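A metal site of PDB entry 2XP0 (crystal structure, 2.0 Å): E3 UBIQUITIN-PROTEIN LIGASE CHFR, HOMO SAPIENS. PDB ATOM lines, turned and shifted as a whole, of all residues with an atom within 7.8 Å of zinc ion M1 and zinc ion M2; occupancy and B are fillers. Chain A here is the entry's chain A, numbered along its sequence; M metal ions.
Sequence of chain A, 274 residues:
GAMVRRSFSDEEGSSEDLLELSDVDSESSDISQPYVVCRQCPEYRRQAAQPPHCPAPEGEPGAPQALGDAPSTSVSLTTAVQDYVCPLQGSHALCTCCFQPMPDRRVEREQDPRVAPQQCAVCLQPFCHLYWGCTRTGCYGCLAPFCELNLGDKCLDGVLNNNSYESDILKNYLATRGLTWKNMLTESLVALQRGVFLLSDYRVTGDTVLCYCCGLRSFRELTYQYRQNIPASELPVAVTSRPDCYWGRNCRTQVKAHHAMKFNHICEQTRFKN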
ATOM      1  N   ARG A  39       5.215   8.629 -34.033  1.00  0.00           N
ATOM      2  CA  ARG A  39       4.717   9.134 -35.316  1.00  0.00           C
ATOM      3  C   ARG A  39       5.340  10.458 -35.759  1.00  0.00           C
ATOM      4  O   ARG A  39       5.506  10.708 -36.943  1.00  0.00           O
ATOM      5  CB  ARG A  39       3.190   9.314 -35.265  1.00  0.00           C
ATOM      6  CG  ARG A  39       2.368   8.067 -35.543  1.00  0.00           C
ATOM      7  CD  ARG A  39       0.891   8.411 -35.646  1.00  0.00           C
ATOM      8  NE  ARG A  39       0.075   7.615 -34.734  1.00  0.00           N
ATOM      9  CZ  ARG A  39      -1.237   7.789 -34.564  1.00  0.00           C
ATOM     10  NH1 ARG A  39      -1.868   8.749 -35.240  1.00  0.00           N
ATOM     11  NH2 ARG A  39      -1.917   7.022 -33.723  1.00  0.00           N
ATOM     12  N   LEU A  94       3.138   7.571 -23.016  1.00  0.00           N
ATOM     13  CA  LEU A  94       2.453   6.478 -23.663  1.00  0.00           C
ATOM     14  C   LEU A  94       0.947   6.612 -23.513  1.00  0.00           C
ATOM     15  O   LEU A  94       0.444   6.870 -22.418  1.00  0.00           O
ATOM     16  CB  LEU A  94       2.929   5.145 -23.091  1.00  0.00           C
ATOM     17  CG  LEU A  94       4.435   4.910 -23.181  1.00  0.00           C
ATOM     18  CD1 LEU A  94       4.786   3.520 -22.646  1.00  0.00           C
ATOM     19  CD2 LEU A  94       4.911   5.057 -24.603  1.00  0.00           C
ATOM     20  N   CYS A  95       0.234   6.460 -24.620  1.00  0.00           N
ATOM     21  CA  CYS A  95      -1.226   6.423 -24.562  1.00  0.00           C
ATOM     22  C   CYS A  95      -1.673   5.257 -23.693  1.00  0.00           C
ATOM     23  O   CYS A  95      -1.293   4.114 -23.927  1.00  0.00           O
ATOM     24  CB  CYS A  95      -1.820   6.306 -25.958  1.00  0.00           C
ATOM     25  SG  CYS A  95      -3.629   6.116 -25.933  1.00  0.00           S
ATOM     26  N   THR A  96      -2.491   5.574 -22.692  1.00  0.00           N
ATOM     27  CA  THR A  96      -3.032   4.575 -21.776  1.00  0.00           C
ATOM     28  C   THR A  96      -3.873   3.501 -22.495  1.00  0.00           C
ATOM     29  O   THR A  96      -4.004   2.382 -22.007  1.00  0.00           O
ATOM     30  CB  THR A  96      -3.900   5.300 -20.719  1.00  0.00           C
ATOM     31  OG1 THR A  96      -3.110   6.314 -20.079  1.00  0.00           O
ATOM     32  CG2 THR A  96      -4.450   4.319 -19.703  1.00  0.00           C
ATOM     33  N   CYS A  97      -4.421   3.857 -23.659  1.00  0.00           N
ATOM     34  CA  CYS A  97      -5.252   2.935 -24.434  1.00  0.00           C
ATOM     35  C   CYS A  97      -4.455   2.021 -25.372  1.00  0.00           C
ATOM     36  O   CYS A  97      -4.585   0.791 -25.309  1.00  0.00           O
ATOM     37  CB  CYS A  97      -6.290   3.717 -25.262  1.00  0.00           C
ATOM     38  SG  CYS A  97      -7.209   2.674 -26.444  1.00  0.00           S
ATOM     39  N   CYS A  98      -3.635   2.601 -26.243  1.00  0.00           N
ATOM     40  CA  CYS A  98      -2.978   1.795 -27.263  1.00  0.00           C
ATOM     41  C   CYS A  98      -1.497   1.524 -26.961  1.00  0.00           C
ATOM     42  O   CYS A  98      -0.830   0.805 -27.698  1.00  0.00           O
ATOM     43  CB  CYS A  98      -3.104   2.473 -28.626  1.00  0.00           C
ATOM     44  SG  CYS A  98      -2.156   3.986 -28.710  1.00  0.00           S
ATOM     45  N   PHE A  99      -0.985   2.123 -25.881  1.00  0.00           N
ATOM     46  CA  PHE A  99       0.402   1.923 -25.439  1.00  0.00           C
ATOM     47  C   PHE A  99       1.460   2.516 -26.369  1.00  0.00           C
ATOM     48  O   PHE A  99       2.653   2.297 -26.183  1.00  0.00           O
ATOM     49  CB  PHE A  99       0.696   0.425 -25.210  1.00  0.00           C
ATOM     50  CG  PHE A  99      -0.362  -0.293 -24.427  1.00  0.00           C
ATOM     51  CD1 PHE A  99      -0.691   0.116 -23.138  1.00  0.00           C
ATOM     52  CD2 PHE A  99      -1.026  -1.382 -24.973  1.00  0.00           C
ATOM     53  CE1 PHE A  99      -1.667  -0.547 -22.415  1.00  0.00           C
ATOM     54  CE2 PHE A  99      -2.011  -2.045 -24.253  1.00  0.00           C
ATOM     55  CZ  PHE A  99      -2.330  -1.626 -22.963  1.00  0.00           C
ATOM     56  N   GLN A 100       1.026   3.287 -27.363  1.00  0.00           N
ATOM     57  CA  GLN A 100       1.971   3.897 -28.298  1.00  0.00           C
ATOM     58  C   GLN A 100       2.401   5.261 -27.788  1.00  0.00           C
ATOM     59  O   GLN A 100       1.595   5.994 -27.212  1.00  0.00           O
ATOM     60  CB  GLN A 100       1.349   4.028 -29.685  1.00  0.00           C
ATOM     61  CG  GLN A 100       0.806   2.728 -30.230  1.00  0.00           C
ATOM     62  CD  GLN A 100       1.848   1.645 -30.299  1.00  0.00           C
ATOM     63  OE1 GLN A 100       2.757   1.708 -31.121  1.00  0.00           O
ATOM     64  NE2 GLN A 100       1.741   0.647 -29.434  1.00  0.00           N
ATOM     65  N   PRO A 101       3.666   5.611 -28.005  1.00  0.00           N
ATOM     66  CA  PRO A 101       4.206   6.911 -27.588  1.00  0.00           C
ATOM     67  C   PRO A 101       3.659   8.063 -28.423  1.00  0.00           C
ATOM     68  O   PRO A 101       3.443   7.922 -29.617  1.00  0.00           O
ATOM     69  CB  PRO A 101       5.699   6.767 -27.868  1.00  0.00           C
ATOM     70  CG  PRO A 101       5.768   5.758 -28.963  1.00  0.00           C
ATOM     71  CD  PRO A 101       4.717   4.766 -28.604  1.00  0.00           C
ATOM     72  N   MET A 102       3.430   9.185 -27.758  1.00  0.00           N
ATOM     73  CA  MET A 102       3.120  10.437 -28.434  1.00  0.00           C
ATOM     74  C   MET A 102       3.953  11.500 -27.726  1.00  0.00           C
ATOM     75  O   MET A 102       4.378  11.312 -26.589  1.00  0.00           O
ATOM     76  CB  MET A 102       1.641  10.761 -28.290  1.00  0.00           C
ATOM     77  CG  MET A 102       1.199  10.970 -26.850  1.00  0.00           C
ATOM     78  SD  MET A 102      -0.574  11.246 -26.636  1.00  0.00           S
ATOM     79  CE  MET A 102      -0.665  11.211 -24.854  1.00  0.00           C
ATOM     80  N   PRO A 126      -2.878   9.812 -19.655  1.00  0.00           N
ATOM     81  CA  PRO A 126      -2.729  10.273 -21.044  1.00  0.00           C
ATOM     82  C   PRO A 126      -3.434   9.364 -22.060  1.00  0.00           C
ATOM     83  O   PRO A 126      -3.400   8.145 -21.918  1.00  0.00           O
ATOM     84  CB  PRO A 126      -1.203  10.219 -21.256  1.00  0.00           C
ATOM     85  CG  PRO A 126      -0.733   9.159 -20.334  1.00  0.00           C
ATOM     86  CD  PRO A 126      -1.634   9.233 -19.112  1.00  0.00           C
ATOM     87  N   PHE A 127      -4.043   9.971 -23.077  1.00  0.00           N
ATOM     88  CA  PHE A 127      -4.630   9.230 -24.195  1.00  0.00           C
ATOM     89  C   PHE A 127      -4.362  10.006 -25.469  1.00  0.00           C
ATOM     90  O   PHE A 127      -4.354  11.229 -25.440  1.00  0.00           O
ATOM     91  CB  PHE A 127      -6.148   9.073 -24.025  1.00  0.00           C
ATOM     92  CG  PHE A 127      -6.546   8.204 -22.879  1.00  0.00           C
ATOM     93  CD1 PHE A 127      -6.778   6.847 -23.077  1.00  0.00           C
ATOM     94  CD2 PHE A 127      -6.696   8.727 -21.622  1.00  0.00           C
ATOM     95  CE1 PHE A 127      -7.158   6.033 -22.020  1.00  0.00           C
ATOM     96  CE2 PHE A 127      -7.055   7.932 -20.563  1.00  0.00           C
ATOM     97  CZ  PHE A 127      -7.287   6.575 -20.761  1.00  0.00           C
ATOM     98  N   CYS A 128      -4.166   9.300 -26.582  1.00  0.00           N
ATOM     99  CA  CYS A 128      -3.697   9.958 -27.806  1.00  0.00           C
ATOM    100  C   CYS A 128      -4.797  10.350 -28.802  1.00  0.00           C
ATOM    101  O   CYS A 128      -4.506  10.984 -29.819  1.00  0.00           O
ATOM    102  CB  CYS A 128      -2.668   9.071 -28.541  1.00  0.00           C
ATOM    103  SG  CYS A 128      -3.370   7.693 -29.501  1.00  0.00           S
ATOM    104  N   HIS A 129      -6.049   9.989 -28.525  1.00  0.00           N
ATOM    105  CA  HIS A 129      -7.054  10.080 -29.584  1.00  0.00           C
ATOM    106  C   HIS A 129      -7.312  11.479 -30.146  1.00  0.00           C
ATOM    107  O   HIS A 129      -7.327  11.655 -31.360  1.00  0.00           O
ATOM    108  CB  HIS A 129      -8.377   9.443 -29.161  1.00  0.00           C
ATOM    109  CG  HIS A 129      -9.328   9.260 -30.313  1.00  0.00           C
ATOM    110  ND1 HIS A 129      -9.026   8.479 -31.402  1.00  0.00           N
ATOM    111  CD2 HIS A 129     -10.581   9.743 -30.523  1.00  0.00           C
ATOM    112  CE1 HIS A 129     -10.057   8.486 -32.241  1.00  0.00           C
ATOM    113  NE2 HIS A 129     -10.999   9.248 -31.732  1.00  0.00           N
ATOM    114  N   LEU A 130      -7.554  12.453 -29.276  1.00  0.00           N
ATOM    115  CA  LEU A 130      -7.849  13.798 -29.754  1.00  0.00           C
ATOM    116  C   LEU A 130      -6.606  14.404 -30.397  1.00  0.00           C
ATOM    117  O   LEU A 130      -6.728  15.207 -31.315  1.00  0.00           O
ATOM    118  CB  LEU A 130      -8.352  14.683 -28.616  1.00  0.00           C
ATOM    119  CG  LEU A 130      -9.766  14.308 -28.185  1.00  0.00           C
ATOM    120  CD1 LEU A 130     -10.207  15.108 -26.981  1.00  0.00           C
ATOM    121  CD2 LEU A 130     -10.726  14.510 -29.347  1.00  0.00           C
ATOM    122  N   TRP A 132      -4.045  12.839 -32.170  1.00  0.00           N
ATOM    123  CA  TRP A 132      -3.756  12.389 -33.536  1.00  0.00           C
ATOM    124  C   TRP A 132      -4.493  11.142 -34.022  1.00  0.00           C
ATOM    125  O   TRP A 132      -4.175  10.610 -35.079  1.00  0.00           O
ATOM    126  CB  TRP A 132      -2.231  12.233 -33.751  1.00  0.00           C
ATOM    127  CG  TRP A 132      -1.555  11.152 -32.923  1.00  0.00           C
ATOM    128  CD1 TRP A 132      -2.152  10.114 -32.272  1.00  0.00           C
ATOM    129  CD2 TRP A 132      -0.145  11.017 -32.689  1.00  0.00           C
ATOM    130  NE1 TRP A 132      -1.203   9.348 -31.633  1.00  0.00           N
ATOM    131  CE2 TRP A 132       0.032   9.880 -31.872  1.00  0.00           C
ATOM    132  CE3 TRP A 132       0.988  11.758 -33.061  1.00  0.00           C
ATOM    133  CZ2 TRP A 132       1.291   9.464 -31.439  1.00  0.00           C
ATOM    134  CZ3 TRP A 132       2.229  11.342 -32.634  1.00  0.00           C
ATOM    135  CH2 TRP A 132       2.376  10.205 -31.826  1.00  0.00           C
ATOM    136  N   GLY A 133      -5.488  10.680 -33.258  1.00  0.00           N
ATOM    137  CA  GLY A 133      -6.277   9.531 -33.671  1.00  0.00           C
ATOM    138  C   GLY A 133      -5.652   8.248 -33.171  1.00  0.00           C
ATOM    139  O   GLY A 133      -4.537   7.898 -33.567  1.00  0.00           O
ATOM    140  N   CYS A 134      -6.352   7.549 -32.295  1.00  0.00           N
ATOM    141  CA  CYS A 134      -5.865   6.308 -31.716  1.00  0.00           C
ATOM    142  C   CYS A 134      -6.486   5.140 -32.478  1.00  0.00           C
ATOM    143  O   CYS A 134      -7.641   5.210 -32.869  1.00  0.00           O
ATOM    144  CB  CYS A 134      -6.283   6.238 -30.237  1.00  0.00           C
ATOM    145  SG  CYS A 134      -5.765   4.733 -29.335  1.00  0.00           S
ATOM    146  N   THR A 135      -5.734   4.075 -32.691  1.00  0.00           N
ATOM    147  CA  THR A 135      -6.288   2.871 -33.331  1.00  0.00           C
ATOM    148  C   THR A 135      -5.957   1.605 -32.551  1.00  0.00           C
ATOM    149  O   THR A 135      -4.786   1.297 -32.302  1.00  0.00           O
ATOM    150  CB  THR A 135      -5.783   2.699 -34.770  1.00  0.00           C
ATOM    151  OG1 THR A 135      -6.208   3.808 -35.561  1.00  0.00           O
ATOM    152  CG2 THR A 135      -6.348   1.420 -35.379  1.00  0.00           C
ATOM    153  N   ARG A 136      -6.998   0.859 -32.171  1.00  0.00           N
ATOM    154  CA  ARG A 136      -6.828  -0.428 -31.519  1.00  0.00           C
ATOM    155  C   ARG A 136      -8.166  -1.131 -31.501  1.00  0.00           C
ATOM    156  O   ARG A 136      -9.203  -0.500 -31.272  1.00  0.00           O
ATOM    157  CB  ARG A 136      -6.321  -0.256 -30.074  1.00  0.00           C
ATOM    158  CG  ARG A 136      -6.163  -1.575 -29.314  1.00  0.00           C
ATOM    159  CD  ARG A 136      -5.641  -1.407 -27.885  1.00  0.00           C
ATOM    160  NE  ARG A 136      -6.585  -0.689 -27.029  1.00  0.00           N
ATOM    161  CZ  ARG A 136      -7.650  -1.238 -26.450  1.00  0.00           C
ATOM    162  NH1 ARG A 136      -7.937  -2.528 -26.634  1.00  0.00           N
ATOM    163  NH2 ARG A 136      -8.449  -0.496 -25.692  1.00  0.00           N
ATOM    164  N   GLY A 138     -11.034  -2.698 -29.945  1.00  0.00           N
ATOM    165  CA  GLY A 138     -11.537  -2.462 -28.613  1.00  0.00           C
ATOM    166  C   GLY A 138     -11.544  -0.979 -28.309  1.00  0.00           C
ATOM    167  O   GLY A 138     -12.232  -0.543 -27.387  1.00  0.00           O
ATOM    168  N   CYS A 139     -10.783  -0.205 -29.074  1.00  0.00           N
ATOM    169  CA  CYS A 139     -10.818   1.250 -28.954  1.00  0.00           C
ATOM    170  C   CYS A 139     -11.891   1.850 -29.853  1.00  0.00           C
ATOM    171  O   CYS A 139     -11.858   1.696 -31.076  1.00  0.00           O
ATOM    172  CB  CYS A 139      -9.460   1.885 -29.250  1.00  0.00           C
ATOM    173  SG  CYS A 139      -9.502   3.702 -29.220  1.00  0.00           S
ATOM    174  N   TYR A 140     -12.842   2.532 -29.215  1.00  0.00           N
ATOM    175  CA  TYR A 140     -13.959   3.161 -29.899  1.00  0.00           C
ATOM    176  C   TYR A 140     -13.669   4.614 -30.265  1.00  0.00           C
ATOM    177  O   TYR A 140     -14.467   5.257 -30.963  1.00  0.00           O
ATOM    178  CB  TYR A 140     -15.185   3.146 -28.991  1.00  0.00           C
ATOM    179  CG  TYR A 140     -15.590   1.770 -28.515  1.00  0.00           C
ATOM    180  CD1 TYR A 140     -15.720   0.708 -29.406  1.00  0.00           C
ATOM    181  CD2 TYR A 140     -15.885   1.534 -27.181  1.00  0.00           C
ATOM    182  CE1 TYR A 140     -16.107  -0.545 -28.980  1.00  0.00           C
ATOM    183  CE2 TYR A 140     -16.268   0.284 -26.733  1.00  0.00           C
ATOM    184  CZ  TYR A 140     -16.374  -0.751 -27.632  1.00  0.00           C
ATOM    185  OH  TYR A 140     -16.773  -1.992 -27.201  1.00  0.00           O
ATOM    186  N   GLY A 141     -12.540   5.130 -29.780  1.00  0.00           N
ATOM    187  CA  GLY A 141     -12.299   6.567 -29.711  1.00  0.00           C
ATOM    188  C   GLY A 141     -12.168   6.962 -28.251  1.00  0.00           C
ATOM    189  O   GLY A 141     -13.133   7.421 -27.618  1.00  0.00           O
ATOM    190  N   CYS A 142     -10.956   6.800 -27.710  1.00  0.00           N
ATOM    191  CA  CYS A 142     -10.747   6.729 -26.266  1.00  0.00           C
ATOM    192  C   CYS A 142     -10.723   8.055 -25.489  1.00  0.00           C
ATOM    193  O   CYS A 142     -10.614   8.036 -24.265  1.00  0.00           O
ATOM    194  CB  CYS A 142      -9.467   5.945 -25.960  1.00  0.00           C
ATOM    195  SG  CYS A 142      -8.015   6.537 -26.845  1.00  0.00           S
ATOM    196  N   LEU A 143     -10.822   9.177 -26.184  1.00  0.00           N
ATOM    197  CA  LEU A 143     -10.850  10.479 -25.513  1.00  0.00           C
ATOM    198  C   LEU A 143     -11.794  11.420 -26.258  1.00  0.00           C
ATOM    199  O   LEU A 143     -11.695  11.547 -27.471  1.00  0.00           O
ATOM    200  CB  LEU A 143      -9.424  11.083 -25.412  1.00  0.00           C
ATOM    201  CG  LEU A 143      -9.209  12.288 -24.481  1.00  0.00           C
ATOM    202  CD1 LEU A 143      -9.410  11.873 -23.021  1.00  0.00           C
ATOM    203  CD2 LEU A 143      -7.840  12.960 -24.674  1.00  0.00           C
ATOM    204  N   TYR A 212     -12.646   6.699 -22.174  1.00  0.00           N
ATOM    205  CA  TYR A 212     -13.649   5.641 -22.254  1.00  0.00           C
ATOM    206  C   TYR A 212     -14.085   5.126 -20.889  1.00  0.00           C
ATOM    207  O   TYR A 212     -15.276   5.100 -20.582  1.00  0.00           O
ATOM    208  CB  TYR A 212     -13.101   4.469 -23.080  1.00  0.00           C
ATOM    209  CG  TYR A 212     -13.985   3.249 -22.979  1.00  0.00           C
ATOM    210  CD1 TYR A 212     -15.212   3.201 -23.623  1.00  0.00           C
ATOM    211  CD2 TYR A 212     -13.591   2.147 -22.220  1.00  0.00           C
ATOM    212  CE1 TYR A 212     -16.028   2.077 -23.529  1.00  0.00           C
ATOM    213  CE2 TYR A 212     -14.388   1.032 -22.123  1.00  0.00           C
ATOM    214  CZ  TYR A 212     -15.604   1.003 -22.767  1.00  0.00           C
ATOM    215  OH  TYR A 212     -16.394  -0.120 -22.656  1.00  0.00           O
HETATM  216 ZN    ZN M   1      -7.620   4.389 -27.927  1.00  0.00          ZN
HETATM  217 ZN    ZN M   2      -3.783   5.744 -28.316  1.00  0.00          ZN
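Within 4 Å of zinc ion M2: Cys 95, Cys 98, Cys 128 and Cys 134.
The nearest printed residue that does not touch zinc ion M2 is Cys 97 (4.4 Å).
Zinc ion M1 is bound by SG of Cys 97 (2.3 Å).
SG of Cys 134 binds zinc ion M1 (2.4 Å).
SG of Cys 139 binds zinc ion M1 (2.4 Å).
The side-chain sulfur (SG) of Cys 142 is bound to zinc ion M1 (2.4 Å).
Zinc ion M1 has four donor atoms within binding distance.
N of Cys 97 sits close to SG of Cys 95 (3.3 Å).
The backbone carbonyl oxygen (O) of Cys 97 sits at hydrogen-bond distance from the guanidinium group (NE) of Arg 136, at 3.0 Å.
The side-chain sulfur (SG) of Cys 128 lies close to the indole nitrogen (NE1) of Trp 132, at 3.5 Å.
The backbone NH (N) of Cys 134 sits at hydrogen-bond distance from a ring nitrogen (ND1) of His 129 (3.0 Å).
The side-chain sulfur (SG) of Cys 139 lies close to the backbone NH (N) of Gly 141.
The backbone NH of Cys 95 is in hydrogen-bond range of the backbone carbonyl oxygen of Gln 100 (3.0 Å).
O of Cys 98 sits at hydrogen-bond distance from NE2 of Gln 100.
The backbone NH (N) of Tyr 212 lies within hydrogen-bond range of the backbone carbonyl oxygen (O) of Cys 142 (3.2 Å).
Four residues have an atom within 4 Å of zinc ion M1: Cys 97, Cys 134, Cys 139 and Cys 142.
The nearest printed residue that does not touch zinc ion M1 is Cys 98 (4.7 Å).
Zinc ion M2 is bound by SG of Cys 128 (2.3 Å), SG of Cys 95 (2.4 Å), SG of Cys 98 (2.4 Å) and SG of Cys 134 (2.4 Å).
Zinc ion M2 has four donor atoms within binding distance.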
